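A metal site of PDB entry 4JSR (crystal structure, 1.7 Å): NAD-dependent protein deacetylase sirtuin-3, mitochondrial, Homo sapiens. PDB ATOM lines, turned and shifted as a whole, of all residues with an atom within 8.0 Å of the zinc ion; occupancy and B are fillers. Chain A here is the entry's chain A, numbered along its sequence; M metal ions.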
ATOM      1  N   THR A 141      19.228  13.874   9.603  1.00  0.00           N
ATOM      2  CA  THR A 141      18.880  14.266  10.954  1.00  0.00           C
ATOM      3  C   THR A 141      20.037  14.945  11.626  1.00  0.00           C
ATOM      4  O   THR A 141      21.148  14.503  11.572  1.00  0.00           O
ATOM      5  CB  THR A 141      18.541  12.971  11.743  1.00  0.00           C
ATOM      6  OG1 THR A 141      17.411  12.323  11.122  1.00  0.00           O
ATOM      7  CG2 THR A 141      18.197  13.263  13.207  1.00  0.00           C
ATOM      8  N   CYS A 142      19.752  15.992  12.435  1.00  0.00           N
ATOM      9  CA  CYS A 142      20.846  16.649  13.209  1.00  0.00           C
ATOM     10  C   CYS A 142      21.358  15.607  14.232  1.00  0.00           C
ATOM     11  O   CYS A 142      20.566  15.030  15.057  1.00  0.00           O
ATOM     12  CB  CYS A 142      20.322  17.923  13.938  1.00  0.00           C
ATOM     13  SG  CYS A 142      21.650  18.627  14.938  1.00  0.00           S
ATOM     14  N   THR A 143      22.678  15.424  14.292  1.00  0.00           N
ATOM     15  CA  THR A 143      23.264  14.476  15.176  1.00  0.00           C
ATOM     16  C   THR A 143      23.231  14.896  16.626  1.00  0.00           C
ATOM     17  O   THR A 143      23.445  14.098  17.550  1.00  0.00           O
ATOM     18  CB  THR A 143      24.711  14.233  14.878  1.00  0.00           C
ATOM     19  OG1 THR A 143      25.484  15.470  14.834  1.00  0.00           O
ATOM     20  CG2 THR A 143      24.801  13.532  13.516  1.00  0.00           C
ATOM     21  N   VAL A 144      22.959  16.168  16.824  1.00  0.00           N
ATOM     22  CA  VAL A 144      22.923  16.745  18.178  1.00  0.00           C
ATOM     23  C   VAL A 144      21.573  16.965  18.743  1.00  0.00           C
ATOM     24  O   VAL A 144      21.336  16.512  19.891  1.00  0.00           O
ATOM     25  CB  VAL A 144      23.734  18.012  18.274  1.00  0.00           C
ATOM     26  CG1 VAL A 144      23.562  18.591  19.685  1.00  0.00           C
ATOM     27  CG2 VAL A 144      25.150  17.673  18.016  1.00  0.00           C
ATOM     28  N   CYS A 145      20.658  17.581  17.992  1.00  0.00           N
ATOM     29  CA  CYS A 145      19.346  17.918  18.570  1.00  0.00           C
ATOM     30  C   CYS A 145      18.258  17.060  17.935  1.00  0.00           C
ATOM     31  O   CYS A 145      17.055  17.104  18.374  1.00  0.00           O
ATOM     32  CB  CYS A 145      18.932  19.389  18.316  1.00  0.00           C
ATOM     33  SG  CYS A 145      18.565  19.836  16.744  1.00  0.00           S
ATOM     34  N   GLN A 146      18.619  16.194  16.946  1.00  0.00           N
ATOM     35  CA  GLN A 146      17.587  15.349  16.288  1.00  0.00           C
ATOM     36  C   GLN A 146      16.553  16.000  15.367  1.00  0.00           C
ATOM     37  O   GLN A 146      15.570  15.383  14.902  1.00  0.00           O
ATOM     38  CB  GLN A 146      16.889  14.422  17.295  1.00  0.00           C
ATOM     39  CG  GLN A 146      17.751  13.649  18.210  1.00  0.00           C
ATOM     40  CD  GLN A 146      16.830  12.830  19.157  1.00  0.00           C
ATOM     41  OE1 GLN A 146      16.306  11.793  18.742  1.00  0.00           O
ATOM     42  NE2 GLN A 146      16.611  13.292  20.409  1.00  0.00           N
ATOM     43  N   ARG A 147      16.753  17.261  14.980  1.00  0.00           N
ATOM     44  CA  ARG A 147      15.885  17.871  14.021  1.00  0.00           C
ATOM     45  C   ARG A 147      16.005  17.180  12.659  1.00  0.00           C
ATOM     46  O   ARG A 147      17.125  16.901  12.223  1.00  0.00           O
ATOM     47  CB  ARG A 147      16.312  19.348  13.866  1.00  0.00           C
ATOM     48  CG  ARG A 147      15.521  20.065  12.841  1.00  0.00           C
ATOM     49  CD  ARG A 147      15.878  21.584  12.796  1.00  0.00           C
ATOM     50  NE  ARG A 147      15.292  22.160  11.601  1.00  0.00           N
ATOM     51  CZ  ARG A 147      15.180  23.454  11.357  1.00  0.00           C
ATOM     52  NH1 ARG A 147      14.677  23.860  10.181  1.00  0.00           N
ATOM     53  NH2 ARG A 147      15.523  24.344  12.270  1.00  0.00           N
ATOM     54  N   PRO A 148      14.908  16.854  12.035  1.00  0.00           N
ATOM     55  CA  PRO A 148      14.876  16.142  10.719  1.00  0.00           C
ATOM     56  C   PRO A 148      14.951  17.161   9.614  1.00  0.00           C
ATOM     57  O   PRO A 148      14.467  18.307   9.753  1.00  0.00           O
ATOM     58  CB  PRO A 148      13.526  15.411  10.749  1.00  0.00           C
ATOM     59  CG  PRO A 148      12.615  16.406  11.614  1.00  0.00           C
ATOM     60  CD  PRO A 148      13.551  16.958  12.682  1.00  0.00           C
ATOM     61  N   PHE A 149      15.579  16.812   8.508  1.00  0.00           N
ATOM     62  CA  PHE A 149      15.600  17.609   7.318  1.00  0.00           C
ATOM     63  C   PHE A 149      15.292  16.755   6.095  1.00  0.00           C
ATOM     64  O   PHE A 149      15.784  15.624   5.958  1.00  0.00           O
ATOM     65  CB  PHE A 149      17.040  18.095   7.082  1.00  0.00           C
ATOM     66  CG  PHE A 149      17.590  18.895   8.161  1.00  0.00           C
ATOM     67  CD1 PHE A 149      17.812  20.239   8.013  1.00  0.00           C
ATOM     68  CD2 PHE A 149      17.981  18.265   9.332  1.00  0.00           C
ATOM     69  CE1 PHE A 149      18.396  21.007   9.091  1.00  0.00           C
ATOM     70  CE2 PHE A 149      18.513  19.001  10.383  1.00  0.00           C
ATOM     71  CZ  PHE A 149      18.738  20.352  10.258  1.00  0.00           C
ATOM     72  N   ARG A 165      25.222  21.720   8.372  1.00  0.00           N
ATOM     73  CA  ARG A 165      25.012  22.067   9.766  1.00  0.00           C
ATOM     74  C   ARG A 165      23.563  22.451  10.156  1.00  0.00           C
ATOM     75  O   ARG A 165      22.824  22.978   9.389  1.00  0.00           O
ATOM     76  CB  ARG A 165      25.923  23.261  10.135  1.00  0.00           C
ATOM     77  CG  ARG A 165      27.392  22.924  10.005  1.00  0.00           C
ATOM     78  CD  ARG A 165      27.954  22.606  11.342  1.00  0.00           C
ATOM     79  NE  ARG A 165      29.336  22.119  11.245  1.00  0.00           N
ATOM     80  CZ  ARG A 165      29.913  21.453  12.195  1.00  0.00           C
ATOM     81  NH1 ARG A 165      29.323  21.321  13.408  1.00  0.00           N
ATOM     82  NH2 ARG A 165      31.113  21.029  12.009  1.00  0.00           N
ATOM     83  N   CYS A 166      23.212  22.163  11.423  1.00  0.00           N
ATOM     84  CA  CYS A 166      21.856  22.427  11.858  1.00  0.00           C
ATOM     85  C   CYS A 166      21.658  23.944  12.182  1.00  0.00           C
ATOM     86  O   CYS A 166      22.499  24.551  12.869  1.00  0.00           O
ATOM     87  CB  CYS A 166      21.738  21.648  13.158  1.00  0.00           C
ATOM     88  SG  CYS A 166      20.073  21.820  13.999  1.00  0.00           S
ATOM     89  N   PRO A 167      20.586  24.478  11.661  1.00  0.00           N
ATOM     90  CA  PRO A 167      20.370  25.966  11.981  1.00  0.00           C
ATOM     91  C   PRO A 167      19.944  26.214  13.418  1.00  0.00           C
ATOM     92  O   PRO A 167      20.071  27.355  13.865  1.00  0.00           O
ATOM     93  CB  PRO A 167      19.272  26.384  11.022  1.00  0.00           C
ATOM     94  CG  PRO A 167      18.535  25.115  10.594  1.00  0.00           C
ATOM     95  CD  PRO A 167      19.545  23.906  10.794  1.00  0.00           C
ATOM     96  N   VAL A 168      19.457  25.205  14.156  1.00  0.00           N
ATOM     97  CA  VAL A 168      19.186  25.354  15.580  1.00  0.00           C
ATOM     98  C   VAL A 168      20.423  25.241  16.487  1.00  0.00           C
ATOM     99  O   VAL A 168      20.700  26.170  17.315  1.00  0.00           O
ATOM    100  CB  VAL A 168      18.112  24.344  16.095  1.00  0.00           C
ATOM    101  CG1 VAL A 168      17.858  24.556  17.692  1.00  0.00           C
ATOM    102  CG2 VAL A 168      16.839  24.437  15.310  1.00  0.00           C
ATOM    103  N   CYS A 169      21.238  24.211  16.382  1.00  0.00           N
ATOM    104  CA  CYS A 169      22.244  23.962  17.363  1.00  0.00           C
ATOM    105  C   CYS A 169      23.640  23.917  16.800  1.00  0.00           C
ATOM    106  O   CYS A 169      24.636  23.692  17.541  1.00  0.00           O
ATOM    107  CB  CYS A 169      21.954  22.755  18.268  1.00  0.00           C
ATOM    108  SG  CYS A 169      22.273  21.204  17.187  1.00  0.00           S
ATOM    109  N   THR A 170      23.694  24.064  15.491  1.00  0.00           N
ATOM    110  CA  THR A 170      24.991  23.991  14.782  1.00  0.00           C
ATOM    111  C   THR A 170      25.619  22.601  14.782  1.00  0.00           C
ATOM    112  O   THR A 170      26.750  22.464  14.382  1.00  0.00           O
ATOM    113  CB  THR A 170      26.046  25.004  15.314  1.00  0.00           C
ATOM    114  OG1 THR A 170      25.328  26.210  15.650  1.00  0.00           O
ATOM    115  CG2 THR A 170      27.071  25.331  14.190  1.00  0.00           C
ATOM    116  N   GLY A 171      24.874  21.559  15.173  1.00  0.00           N
ATOM    117  CA  GLY A 171      25.466  20.225  14.993  1.00  0.00           C
ATOM    118  C   GLY A 171      25.557  19.753  13.582  1.00  0.00           C
ATOM    119  O   GLY A 171      24.882  20.252  12.677  1.00  0.00           O
ATOM    120  N   VAL A 172      26.409  18.749  13.392  1.00  0.00           N
ATOM    121  CA  VAL A 172      26.442  18.170  12.052  1.00  0.00           C
ATOM    122  C   VAL A 172      25.143  17.445  11.666  1.00  0.00           C
ATOM    123  O   VAL A 172      24.578  16.696  12.513  1.00  0.00           O
ATOM    124  CB  VAL A 172      27.559  17.159  12.065  1.00  0.00           C
ATOM    125  CG1 VAL A 172      27.529  16.256  10.721  1.00  0.00           C
ATOM    126  CG2 VAL A 172      28.935  17.933  12.087  1.00  0.00           C
ATOM    127  N   VAL A 173      24.644  17.646  10.462  1.00  0.00           N
ATOM    128  CA  VAL A 173      23.420  16.964   9.999  1.00  0.00           C
ATOM    129  C   VAL A 173      23.826  15.766   9.174  1.00  0.00           C
ATOM    130  O   VAL A 173      24.473  15.978   8.173  1.00  0.00           O
ATOM    131  CB  VAL A 173      22.606  17.897   9.130  1.00  0.00           C
ATOM    132  CG1 VAL A 173      21.328  17.263   8.519  1.00  0.00           C
ATOM    133  CG2 VAL A 173      22.175  19.098  10.115  1.00  0.00           C
HETATM  134 ZN    ZN M   1      20.558  20.493  15.760  1.00  0.00          ZN
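The zinc ion is bound by SG of Cys 166 (2.3 Å), SG of Cys 142 (2.3 Å), SG of Cys 145 (2.3 Å) and SG of Cys 169 (2.3 Å). The zinc ion has four donor atoms within binding distance.
The nearest printed residue that does not touch the zinc ion is Gly 171 (4.5 Å).
The backbone NH (N) of Cys 166 lies within hydrogen-bond range of the backbone carbonyl oxygen (O) of Gly 171 (2.8 Å). N of Cys 142 sits at hydrogen-bond distance from O of Arg 147 (2.8 Å). SG of Cys 166 sits close to N of Val 168 (3.4 Å). The side-chain sulfur (SG) of Cys 169 sits close to the backbone NH (N) of Gly 171 (3.3 Å). The side-chain sulfur of Cys 145 lies close to the backbone NH of Arg 147 (3.6 Å). SG of Cys 142 lies close to N of Val 144 (3.4 Å).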
